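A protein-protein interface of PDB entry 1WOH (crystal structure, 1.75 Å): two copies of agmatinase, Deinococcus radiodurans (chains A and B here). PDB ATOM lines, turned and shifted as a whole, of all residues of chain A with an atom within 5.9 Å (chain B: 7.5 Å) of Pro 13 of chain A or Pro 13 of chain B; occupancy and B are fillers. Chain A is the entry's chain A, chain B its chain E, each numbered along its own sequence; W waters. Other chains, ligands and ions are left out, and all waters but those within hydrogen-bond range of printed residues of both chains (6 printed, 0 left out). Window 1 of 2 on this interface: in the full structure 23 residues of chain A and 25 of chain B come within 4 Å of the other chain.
The guanidinium group of Arg 53 of chain B sits at hydrogen-bond distance from the backbone carbonyl oxygen of Gly 11 of chain A (2.9 Å).
The backbone NH of Gly 11 of chain A is in hydrogen-bond range of the side-chain carboxylate of Asp 85 of chain B (2.7 Å).
The guanidinium group of Arg 53 of chain A is in hydrogen-bond range of the backbone carbonyl oxygen of Pro 8 of chain B (3.2 Å).
The guanidinium group (NH2) of Arg 53 of chain A sits at hydrogen-bond distance from the backbone carbonyl oxygen (O) of Gly 10 of chain B, 3.5 Å away.
The backbone carbonyl oxygen (O) of Gly 11 of chain B lies within hydrogen-bond range of the guanidinium group (NH2) of Arg 53 of chain A (3.0 Å).
The side-chain carboxylate (OE1) of Glu 57 of chain B lies close to the side-chain carboxylate (OE1) of Glu 57 of chain A.
OD2 of Asp 82 of chain A lies within hydrogen-bond range of N of Phe 15 of chain A.
The guanidinium group of Arg 56 of chain A is in salt-bridge range of the side-chain carboxylate of Asp 82 of chain A (2.7 Å).
The backbone carbonyl oxygen (O) of Gly 10 of chain B is in hydrogen-bond range of the guanidinium group (NH1) of Arg 17 of chain B (2.8 Å).
The backbone NH (N) of Phe 15 of chain B is in hydrogen-bond range of the side-chain carboxylate (OD2) of Asp 82 of chain B, 2.7 Å away.
O of Arg 56 of chain B is in hydrogen-bond range of OG of Ser 59 of chain B (2.6 Å).
The side-chain carboxylate (OD2) of Asp 82 of chain B is in salt-bridge range of the guanidinium group (NE) of Arg 56 of chain B, at 2.8 Å.
Among the printed residues, pairs that only touch across the chains: Ile 12 of chain A with Arg 56 of chain B (3.2 Å), Arg 53 of chain A with Leu 60 of chain B (3.2 Å), Arg 56 of chain A with Ile 12 of chain B (3.3 Å), Ile 12 of chain A with Ile 12 of chain B (3.5 Å), Leu 60 of chain A with Arg 53 of chain B (3.5 Å), Ile 12 of chain A with Leu 20 of chain B (3.7 Å), Asp 82 of chain A with Ile 12 of chain B (3.8 Å), Pro 13 of chain A with Pro 13 of chain B (3.8 Å), Ile 12 of chain A with Asp 82 of chain B (3.9 Å), Pro 13 of chain A with Arg 53 of chain B (3.9 Å), Arg 53 of chain A with Glu 57 of chain B (3.9 Å), Pro 13 of chain A with Ile 12 of chain B (3.9 Å), Glu 57 of chain A with Arg 53 of chain B (3.97 Å) and Ile 12 of chain A with Pro 13 of chain B (3.997 Å).
Of chain B, only Ile 12, Pro 13 and Arg 53 come within 4 Å of Pro 13 of chain A.
Printed residues of chain A within 4 Å of Pro 13 of chain B: Ile 12 and Pro 13.
Of the printed residues of chain A, Pro 8 of chain B touches Arg 53.
Printed residues of chain B within 4 Å of Glu 57 of chain A: Arg 53 (3.97 Å) and Glu 57 (2.4 Å).
The nearest printed residue of chain A that does not touch Pro 13 of chain B is Arg 53 of chain A (4.1 Å).
Printed residues of chain B that touch a printed residue of chain A: Pro 8, Gly 10, Gly 11, Ile 12, Pro 13, Leu 20, Arg 53, Arg 56, Glu 57, Leu 60, Asp 82 and Asp 85.
Of the 10 printed residues of chain A, 8 touch a printed residue of chain B.
Hydrophobic or aromatic side chains of chain A that line the printed part of chain B: Ile 12, Pro 13 and Leu 60.
Along chain A the printed residues that touch a printed residue of chain B span positions 11 to 82.
Among the printed residues, no Asp or Glu carboxylate lies within 4 Å of a Lys or Arg side-chain nitrogen of the other chain.
Gly 11 of chain A touches Arg 53 of chain B, and with the chains exchanged Arg 53 of chain A touches Gly 11 of chain B.
Ile 12 of chain A touches Pro 13 of chain B, and with the chains exchanged Pro 13 of chain A touches Ile 12 of chain B.
Ile 12 of chain A touches Arg 56 of chain B, and with the chains exchanged Arg 56 of chain A touches Ile 12 of chain B.
Ile 12 of chain A touches Asp 82 of chain B, and with the chains exchanged Asp 82 of chain A touches Ile 12 of chain B.
Of the 20 pairs that touch across the chains among the printed residues, 15 have their exchanged pair printed and touching as well.
Water W6 bridges the guanidinium group of Arg 53 of chain A and the side-chain carboxylate of Glu 57 of chain B.
Water W1 bridges O of Glu 57 of chain A and NH1 of Arg 53 of chain B.
Water W5 bridges NH1 of Arg 53 of chain B and OE2 of Glu 57 of chain A.
Water W2 lies within hydrogen-bond range of O of Gly 11 of chain B, NE of Arg 53 of chain A and NH1 of Arg 56 of chain A.
Water W4 lies within hydrogen-bond range of the backbone carbonyl oxygen (O) of Pro 8 of chain B (2.8 Å), the backbone carbonyl oxygen (O) of Glu 57 of chain B (2.9 Å) and the guanidinium group (NH1) of Arg 53 of chain A (3.2 Å).
Water W3 lies within hydrogen-bond range of O of Gly 11 of chain A, NH1 of Arg 56 of chain B and NE of Arg 53 of chain B.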
ATOM      1  N   GLY A  11     -23.529  -8.606  24.210  1.00  0.00           N
ATOM      2  CA  GLY A  11     -24.904  -8.453  23.767  1.00  0.00           C
ATOM      3  C   GLY A  11     -25.675  -7.356  24.477  1.00  0.00           C
ATOM      4  O   GLY A  11     -25.216  -6.802  25.478  1.00  0.00           O
ATOM      5  N   ILE A  12     -26.847  -7.034  23.940  1.00  0.00           N
ATOM      6  CA  ILE A  12     -27.704  -6.015  24.530  1.00  0.00           C
ATOM      7  C   ILE A  12     -28.378  -6.626  25.752  1.00  0.00           C
ATOM      8  O   ILE A  12     -29.003  -7.683  25.668  1.00  0.00           O
ATOM      9  CB  ILE A  12     -28.801  -5.565  23.548  1.00  0.00           C
ATOM     10  CG1 ILE A  12     -28.170  -5.097  22.233  1.00  0.00           C
ATOM     11  CG2 ILE A  12     -29.618  -4.440  24.173  1.00  0.00           C
ATOM     12  CD1 ILE A  12     -27.220  -3.926  22.387  1.00  0.00           C
ATOM     13  N   PRO A  13     -28.267  -5.967  26.910  1.00  0.00           N
ATOM     14  CA  PRO A  13     -28.896  -6.520  28.108  1.00  0.00           C
ATOM     15  C   PRO A  13     -30.422  -6.422  28.184  1.00  0.00           C
ATOM     16  O   PRO A  13     -30.974  -5.353  28.434  1.00  0.00           O
ATOM     17  CB  PRO A  13     -28.210  -5.751  29.234  1.00  0.00           C
ATOM     18  CG  PRO A  13     -27.975  -4.416  28.618  1.00  0.00           C
ATOM     19  CD  PRO A  13     -27.468  -4.772  27.235  1.00  0.00           C
ATOM     20  N   THR A  14     -31.092  -7.547  27.939  1.00  0.00           N
ATOM     21  CA  THR A  14     -32.545  -7.633  28.051  1.00  0.00           C
ATOM     22  C   THR A  14     -32.723  -8.703  29.110  1.00  0.00           C
ATOM     23  O   THR A  14     -31.840  -9.548  29.287  1.00  0.00           O
ATOM     24  CB  THR A  14     -33.238  -8.058  26.732  1.00  0.00           C
ATOM     25  OG1 THR A  14     -32.650  -9.264  26.229  1.00  0.00           O
ATOM     26  CG2 THR A  14     -33.117  -6.957  25.701  1.00  0.00           C
ATOM     27  N   PHE A  15     -33.834  -8.676  29.835  1.00  0.00           N
ATOM     28  CA  PHE A  15     -34.000  -9.661  30.892  1.00  0.00           C
ATOM     29  C   PHE A  15     -33.972 -11.091  30.362  1.00  0.00           C
ATOM     30  O   PHE A  15     -34.761 -11.452  29.490  1.00  0.00           O
ATOM     31  CB  PHE A  15     -35.288  -9.425  31.678  1.00  0.00           C
ATOM     32  CG  PHE A  15     -35.278 -10.080  33.024  1.00  0.00           C
ATOM     33  CD1 PHE A  15     -34.422  -9.619  34.021  1.00  0.00           C
ATOM     34  CD2 PHE A  15     -36.059 -11.205  33.276  1.00  0.00           C
ATOM     35  CE1 PHE A  15     -34.336 -10.274  35.250  1.00  0.00           C
ATOM     36  CE2 PHE A  15     -35.986 -11.869  34.494  1.00  0.00           C
ATOM     37  CZ  PHE A  15     -35.119 -11.405  35.488  1.00  0.00           C
ATOM     38  N   ARG A  53     -32.103  -1.831  34.976  1.00  0.00           N
ATOM     39  CA  ARG A  53     -30.986  -2.024  34.058  1.00  0.00           C
ATOM     40  C   ARG A  53     -29.956  -2.997  34.626  1.00  0.00           C
ATOM     41  O   ARG A  53     -29.490  -3.904  33.935  1.00  0.00           O
ATOM     42  CB  ARG A  53     -30.332  -0.673  33.743  1.00  0.00           C
ATOM     43  CG  ARG A  53     -29.232  -0.728  32.700  1.00  0.00           C
ATOM     44  CD  ARG A  53     -28.941   0.667  32.159  1.00  0.00           C
ATOM     45  NE  ARG A  53     -30.077   1.210  31.413  1.00  0.00           N
ATOM     46  CZ  ARG A  53     -30.157   2.467  30.985  1.00  0.00           C
ATOM     47  NH1 ARG A  53     -29.165   3.318  31.232  1.00  0.00           N
ATOM     48  NH2 ARG A  53     -31.223   2.874  30.306  1.00  0.00           N
ATOM     49  N   ARG A  56     -31.188  -6.579  34.455  1.00  0.00           N
ATOM     50  CA  ARG A  56     -31.122  -7.156  33.115  1.00  0.00           C
ATOM     51  C   ARG A  56     -29.687  -7.612  32.859  1.00  0.00           C
ATOM     52  O   ARG A  56     -29.444  -8.745  32.436  1.00  0.00           O
ATOM     53  CB  ARG A  56     -31.541  -6.128  32.057  1.00  0.00           C
ATOM     54  CG  ARG A  56     -33.022  -5.754  32.102  1.00  0.00           C
ATOM     55  CD  ARG A  56     -33.392  -4.795  30.975  1.00  0.00           C
ATOM     56  NE  ARG A  56     -34.840  -4.692  30.812  1.00  0.00           N
ATOM     57  CZ  ARG A  56     -35.593  -3.701  31.278  1.00  0.00           C
ATOM     58  NH1 ARG A  56     -35.045  -2.688  31.951  1.00  0.00           N
ATOM     59  NH2 ARG A  56     -36.905  -3.720  31.066  1.00  0.00           N
ATOM     60  N   GLU A  57     -28.734  -6.727  33.120  1.00  0.00           N
ATOM     61  CA  GLU A  57     -27.331  -7.069  32.927  1.00  0.00           C
ATOM     62  C   GLU A  57     -26.990  -8.319  33.737  1.00  0.00           C
ATOM     63  O   GLU A  57     -26.374  -9.256  33.222  1.00  0.00           O
ATOM     64  CB  GLU A  57     -26.439  -5.902  33.367  1.00  0.00           C
ATOM     65  CG  GLU A  57     -26.666  -4.626  32.572  1.00  0.00           C
ATOM     66  CD  GLU A  57     -25.927  -3.424  33.145  1.00  0.00           C
ATOM     67  OE1 GLU A  57     -26.025  -2.333  32.551  1.00  0.00           O
ATOM     68  OE2 GLU A  57     -25.254  -3.564  34.188  1.00  0.00           O
ATOM     69  N   LEU A  60     -28.051 -11.945  32.582  1.00  0.00           N
ATOM     70  CA  LEU A  60     -27.322 -12.615  31.513  1.00  0.00           C
ATOM     71  C   LEU A  60     -26.462 -13.729  32.108  1.00  0.00           C
ATOM     72  O   LEU A  60     -25.935 -14.572  31.388  1.00  0.00           O
ATOM     73  CB  LEU A  60     -26.462 -11.617  30.729  1.00  0.00           C
ATOM     74  CG  LEU A  60     -27.263 -10.494  30.054  1.00  0.00           C
ATOM     75  CD1 LEU A  60     -26.354  -9.686  29.137  1.00  0.00           C
ATOM     76  CD2 LEU A  60     -28.418 -11.087  29.262  1.00  0.00           C
ATOM     77  N   ASP A  82     -39.101  -9.186  26.928  1.00  0.00           N
ATOM     78  CA  ASP A  82     -38.750  -8.018  27.736  1.00  0.00           C
ATOM     79  C   ASP A  82     -39.534  -6.857  27.138  1.00  0.00           C
ATOM     80  O   ASP A  82     -39.227  -6.406  26.036  1.00  0.00           O
ATOM     81  CB  ASP A  82     -37.243  -7.730  27.658  1.00  0.00           C
ATOM     82  CG  ASP A  82     -36.811  -6.634  28.619  1.00  0.00           C
ATOM     83  OD1 ASP A  82     -37.634  -5.735  28.888  1.00  0.00           O
ATOM     84  OD2 ASP A  82     -35.657  -6.663  29.098  1.00  0.00           O
ATOM     85  N   PRO B   8     -32.467   9.232  30.467  1.00  0.00           N
ATOM     86  CA  PRO B   8     -31.285   8.387  30.259  1.00  0.00           C
ATOM     87  C   PRO B   8     -31.278   7.057  31.018  1.00  0.00           C
ATOM     88  O   PRO B   8     -30.727   6.059  30.533  1.00  0.00           O
ATOM     89  CB  PRO B   8     -30.136   9.299  30.677  1.00  0.00           C
ATOM     90  CG  PRO B   8     -30.642  10.651  30.295  1.00  0.00           C
ATOM     91  CD  PRO B   8     -32.074  10.616  30.779  1.00  0.00           C
ATOM     92  N   GLY B  10     -33.822   5.230  31.590  1.00  0.00           N
ATOM     93  CA  GLY B  10     -34.920   4.380  31.171  1.00  0.00           C
ATOM     94  C   GLY B  10     -34.749   3.714  29.817  1.00  0.00           C
ATOM     95  O   GLY B  10     -34.078   4.244  28.932  1.00  0.00           O
ATOM     96  N   GLY B  11     -35.355   2.538  29.673  1.00  0.00           N
ATOM     97  CA  GLY B  11     -35.299   1.801  28.426  1.00  0.00           C
ATOM     98  C   GLY B  11     -34.100   0.894  28.252  1.00  0.00           C
ATOM     99  O   GLY B  11     -33.148   0.943  29.031  1.00  0.00           O
ATOM    100  N   ILE B  12     -34.152   0.057  27.218  1.00  0.00           N
ATOM    101  CA  ILE B  12     -33.063  -0.857  26.916  1.00  0.00           C
ATOM    102  C   ILE B  12     -31.949  -0.017  26.305  1.00  0.00           C
ATOM    103  O   ILE B  12     -32.187   0.792  25.404  1.00  0.00           O
ATOM    104  CB  ILE B  12     -33.498  -1.935  25.906  1.00  0.00           C
ATOM    105  CG1 ILE B  12     -34.749  -2.653  26.420  1.00  0.00           C
ATOM    106  CG2 ILE B  12     -32.362  -2.921  25.678  1.00  0.00           C
ATOM    107  CD1 ILE B  12     -34.584  -3.293  27.786  1.00  0.00           C
ATOM    108  N   PRO B  13     -30.718  -0.188  26.794  1.00  0.00           N
ATOM    109  CA  PRO B  13     -29.612   0.597  26.258  1.00  0.00           C
ATOM    110  C   PRO B  13     -28.997   0.108  24.954  1.00  0.00           C
ATOM    111  O   PRO B  13     -28.165  -0.798  24.946  1.00  0.00           O
ATOM    112  CB  PRO B  13     -28.612   0.588  27.404  1.00  0.00           C
ATOM    113  CG  PRO B  13     -28.775  -0.789  27.949  1.00  0.00           C
ATOM    114  CD  PRO B  13     -30.288  -0.963  27.972  1.00  0.00           C
ATOM    115  N   THR B  14     -29.431   0.709  23.854  1.00  0.00           N
ATOM    116  CA  THR B  14     -28.879   0.415  22.541  1.00  0.00           C
ATOM    117  C   THR B  14     -28.235   1.744  22.159  1.00  0.00           C
ATOM    118  O   THR B  14     -28.658   2.800  22.630  1.00  0.00           O
ATOM    119  CB  THR B  14     -29.964   0.049  21.511  1.00  0.00           C
ATOM    120  OG1 THR B  14     -30.904   1.124  21.388  1.00  0.00           O
ATOM    121  CG2 THR B  14     -30.685  -1.222  21.933  1.00  0.00           C
ATOM    122  N   PHE B  15     -27.210   1.703  21.321  1.00  0.00           N
ATOM    123  CA  PHE B  15     -26.529   2.930  20.937  1.00  0.00           C
ATOM    124  C   PHE B  15     -27.476   3.949  20.316  1.00  0.00           C
ATOM    125  O   PHE B  15     -28.231   3.624  19.402  1.00  0.00           O
ATOM    126  CB  PHE B  15     -25.389   2.629  19.962  1.00  0.00           C
ATOM    127  CG  PHE B  15     -24.382   3.730  19.877  1.00  0.00           C
ATOM    128  CD1 PHE B  15     -23.515   3.972  20.936  1.00  0.00           C
ATOM    129  CD2 PHE B  15     -24.335   4.564  18.768  1.00  0.00           C
ATOM    130  CE1 PHE B  15     -22.617   5.031  20.895  1.00  0.00           C
ATOM    131  CE2 PHE B  15     -23.442   5.625  18.716  1.00  0.00           C
ATOM    132  CZ  PHE B  15     -22.581   5.860  19.781  1.00  0.00           C
ATOM    133  N   ALA B  16     -27.422   5.180  20.817  1.00  0.00           N
ATOM    134  CA  ALA B  16     -28.261   6.271  20.327  1.00  0.00           C
ATOM    135  C   ALA B  16     -29.742   5.911  20.419  1.00  0.00           C
ATOM    136  O   ALA B  16     -30.591   6.520  19.757  1.00  0.00           O
ATOM    137  CB  ALA B  16     -27.885   6.606  18.888  1.00  0.00           C
ATOM    138  N   ARG B  17     -30.035   4.922  21.259  1.00  0.00           N
ATOM    139  CA  ARG B  17     -31.383   4.419  21.471  1.00  0.00           C
ATOM    140  C   ARG B  17     -31.952   3.938  20.132  1.00  0.00           C
ATOM    141  O   ARG B  17     -33.144   4.040  19.862  1.00  0.00           O
ATOM    142  CB  ARG B  17     -32.275   5.506  22.105  1.00  0.00           C
ATOM    143  CG  ARG B  17     -33.389   4.938  22.989  1.00  0.00           C
ATOM    144  CD  ARG B  17     -34.298   6.013  23.592  1.00  0.00           C
ATOM    145  NE  ARG B  17     -33.774   6.629  24.812  1.00  0.00           N
ATOM    146  CZ  ARG B  17     -33.685   6.021  25.996  1.00  0.00           C
ATOM    147  NH1 ARG B  17     -34.082   4.761  26.144  1.00  0.00           N
ATOM    148  NH2 ARG B  17     -33.206   6.681  27.045  1.00  0.00           N
ATOM    149  N   ALA B  18     -31.076   3.389  19.301  1.00  0.00           N
ATOM    150  CA  ALA B  18     -31.470   2.894  17.987  1.00  0.00           C
ATOM    151  C   ALA B  18     -32.063   1.492  18.044  1.00  0.00           C
ATOM    152  O   ALA B  18     -31.765   0.707  18.949  1.00  0.00           O
ATOM    153  CB  ALA B  18     -30.265   2.900  17.056  1.00  0.00           C
ATOM    154  N   LEU B  20     -32.708  -2.407  17.576  1.00  0.00           N
ATOM    155  CA  LEU B  20     -31.765  -3.511  17.554  1.00  0.00           C
ATOM    156  C   LEU B  20     -31.941  -4.357  16.297  1.00  0.00           C
ATOM    157  O   LEU B  20     -33.062  -4.665  15.891  1.00  0.00           O
ATOM    158  CB  LEU B  20     -31.947  -4.387  18.797  1.00  0.00           C
ATOM    159  CG  LEU B  20     -31.050  -5.627  18.896  1.00  0.00           C
ATOM    160  CD1 LEU B  20     -29.583  -5.219  18.863  1.00  0.00           C
ATOM    161  CD2 LEU B  20     -31.361  -6.379  20.179  1.00  0.00           C
ATOM    162  N   PRO B  52     -18.382  -1.423  25.460  1.00  0.00           N
ATOM    163  CA  PRO B  52     -19.517  -1.330  24.540  1.00  0.00           C
ATOM    164  C   PRO B  52     -20.826  -1.073  25.262  1.00  0.00           C
ATOM    165  O   PRO B  52     -21.634  -0.274  24.814  1.00  0.00           O
ATOM    166  CB  PRO B  52     -19.495  -2.681  23.828  1.00  0.00           C
ATOM    167  CG  PRO B  52     -18.019  -2.994  23.788  1.00  0.00           C
ATOM    168  CD  PRO B  52     -17.579  -2.629  25.192  1.00  0.00           C
ATOM    169  N   ARG B  53     -21.022  -1.749  26.392  1.00  0.00           N
ATOM    170  CA  ARG B  53     -22.243  -1.586  27.169  1.00  0.00           C
ATOM    171  C   ARG B  53     -22.276  -0.207  27.822  1.00  0.00           C
ATOM    172  O   ARG B  53     -23.304   0.468  27.802  1.00  0.00           O
ATOM    173  CB  ARG B  53     -22.341  -2.684  28.234  1.00  0.00           C
ATOM    174  CG  ARG B  53     -23.656  -2.699  29.003  1.00  0.00           C
ATOM    175  CD  ARG B  53     -23.846  -4.037  29.704  1.00  0.00           C
ATOM    176  NE  ARG B  53     -23.924  -5.126  28.733  1.00  0.00           N
ATOM    177  CZ  ARG B  53     -23.874  -6.418  29.043  1.00  0.00           C
ATOM    178  NH1 ARG B  53     -23.748  -6.802  30.307  1.00  0.00           N
ATOM    179  NH2 ARG B  53     -23.938  -7.326  28.081  1.00  0.00           N
ATOM    180  N   ALA B  54     -21.151   0.212  28.389  1.00  0.00           N
ATOM    181  CA  ALA B  54     -21.073   1.523  29.034  1.00  0.00           C
ATOM    182  C   ALA B  54     -21.308   2.633  28.015  1.00  0.00           C
ATOM    183  O   ALA B  54     -21.980   3.620  28.311  1.00  0.00           O
ATOM    184  CB  ALA B  54     -19.719   1.702  29.707  1.00  0.00           C
ATOM    185  N   LEU B  55     -20.761   2.473  26.811  1.00  0.00           N
ATOM    186  CA  LEU B  55     -20.938   3.476  25.764  1.00  0.00           C
ATOM    187  C   LEU B  55     -22.397   3.551  25.318  1.00  0.00           C
ATOM    188  O   LEU B  55     -22.929   4.639  25.079  1.00  0.00           O
ATOM    189  CB  LEU B  55     -20.027   3.160  24.575  1.00  0.00           C
ATOM    190  CG  LEU B  55     -18.553   3.468  24.864  1.00  0.00           C
ATOM    191  CD1 LEU B  55     -17.661   2.798  23.830  1.00  0.00           C
ATOM    192  CD2 LEU B  55     -18.340   4.985  24.866  1.00  0.00           C
ATOM    193  N   ARG B  56     -23.049   2.396  25.213  1.00  0.00           N
ATOM    194  CA  ARG B  56     -24.449   2.372  24.824  1.00  0.00           C
ATOM    195  C   ARG B  56     -25.275   3.116  25.865  1.00  0.00           C
ATOM    196  O   ARG B  56     -26.126   3.937  25.529  1.00  0.00           O
ATOM    197  CB  ARG B  56     -24.955   0.939  24.710  1.00  0.00           C
ATOM    198  CG  ARG B  56     -24.415   0.188  23.505  1.00  0.00           C
ATOM    199  CD  ARG B  56     -25.148  -1.133  23.331  1.00  0.00           C
ATOM    200  NE  ARG B  56     -24.886  -1.716  22.020  1.00  0.00           N
ATOM    201  CZ  ARG B  56     -23.909  -2.580  21.760  1.00  0.00           C
ATOM    202  NH1 ARG B  56     -23.090  -2.981  22.727  1.00  0.00           N
ATOM    203  NH2 ARG B  56     -23.740  -3.031  20.523  1.00  0.00           N
ATOM    204  N   GLU B  57     -25.023   2.810  27.132  1.00  0.00           N
ATOM    205  CA  GLU B  57     -25.742   3.452  28.223  1.00  0.00           C
ATOM    206  C   GLU B  57     -25.493   4.962  28.218  1.00  0.00           C
ATOM    207  O   GLU B  57     -26.432   5.748  28.340  1.00  0.00           O
ATOM    208  CB  GLU B  57     -25.311   2.839  29.562  1.00  0.00           C
ATOM    209  CG  GLU B  57     -25.652   1.355  29.677  1.00  0.00           C
ATOM    210  CD  GLU B  57     -25.097   0.704  30.934  1.00  0.00           C
ATOM    211  OE1 GLU B  57     -25.346  -0.503  31.131  1.00  0.00           O
ATOM    212  OE2 GLU B  57     -24.414   1.393  31.723  1.00  0.00           O
ATOM    213  N   ALA B  58     -24.235   5.359  28.059  1.00  0.00           N
ATOM    214  CA  ALA B  58     -23.882   6.778  28.042  1.00  0.00           C
ATOM    215  C   ALA B  58     -24.478   7.500  26.838  1.00  0.00           C
ATOM    216  O   ALA B  58     -24.750   8.700  26.903  1.00  0.00           O
ATOM    217  CB  ALA B  58     -22.361   6.947  28.054  1.00  0.00           C
ATOM    218  N   SER B  59     -24.695   6.774  25.743  1.00  0.00           N
ATOM    219  CA  SER B  59     -25.254   7.393  24.545  1.00  0.00           C
ATOM    220  C   SER B  59     -26.707   7.841  24.748  1.00  0.00           C
ATOM    221  O   SER B  59     -27.218   8.659  23.987  1.00  0.00           O
ATOM    222  CB  SER B  59     -25.172   6.431  23.345  1.00  0.00           C
ATOM    223  OG  SER B  59     -26.186   5.439  23.393  1.00  0.00           O
ATOM    224  N   LEU B  60     -27.375   7.317  25.772  1.00  0.00           N
ATOM    225  CA  LEU B  60     -28.754   7.717  26.018  1.00  0.00           C
ATOM    226  C   LEU B  60     -28.808   9.188  26.438  1.00  0.00           C
ATOM    227  O   LEU B  60     -29.878   9.787  26.496  1.00  0.00           O
ATOM    228  CB  LEU B  60     -29.398   6.820  27.079  1.00  0.00           C
ATOM    229  CG  LEU B  60     -29.449   5.341  26.677  1.00  0.00           C
ATOM    230  CD1 LEU B  60     -30.217   4.541  27.714  1.00  0.00           C
ATOM    231  CD2 LEU B  60     -30.126   5.210  25.310  1.00  0.00           C
ATOM    232  N   ASP B  82     -28.591  -0.551  15.827  1.00  0.00           N
ATOM    233  CA  ASP B  82     -27.608  -1.149  16.726  1.00  0.00           C
ATOM    234  C   ASP B  82     -27.574  -2.635  16.399  1.00  0.00           C
ATOM    235  O   ASP B  82     -28.548  -3.350  16.633  1.00  0.00           O
ATOM    236  CB  ASP B  82     -28.002  -0.951  18.195  1.00  0.00           C
ATOM    237  CG  ASP B  82     -26.894  -1.360  19.153  1.00  0.00           C
ATOM    238  OD1 ASP B  82     -26.145  -2.306  18.834  1.00  0.00           O
ATOM    239  OD2 ASP B  82     -26.780  -0.747  20.236  1.00  0.00           O
ATOM    240  N   ASP B  85     -23.536  -7.058  19.622  1.00  0.00           N
ATOM    241  CA  ASP B  85     -22.112  -7.374  19.739  1.00  0.00           C
ATOM    242  C   ASP B  85     -21.707  -8.613  18.956  1.00  0.00           C
ATOM    243  O   ASP B  85     -22.521  -9.504  18.704  1.00  0.00           O
ATOM    244  CB  ASP B  85     -21.718  -7.636  21.200  1.00  0.00           C
ATOM    245  CG  ASP B  85     -21.877  -6.416  22.087  1.00  0.00           C
ATOM    246  OD1 ASP B  85     -21.863  -5.286  21.558  1.00  0.00           O
ATOM    247  OD2 ASP B  85     -22.001  -6.598  23.317  1.00  0.00           O
HETATM  248  O   HOH W   1     -23.766  -9.256  32.476  1.00  0.00           O
HETATM  249  O   HOH W   2     -32.412  -0.902  30.980  1.00  0.00           O
HETATM  250  O   HOH W   3     -24.220  -3.921  25.600  1.00  0.00           O
HETATM  251  O   HOH W   4     -27.927   6.248  30.825  1.00  0.00           O
HETATM  252  O   HOH W   5     -23.164  -5.277  32.520  1.00  0.00           O
HETATM  253  O   HOH W   6     -26.988   3.062  32.796  1.00  0.00           O
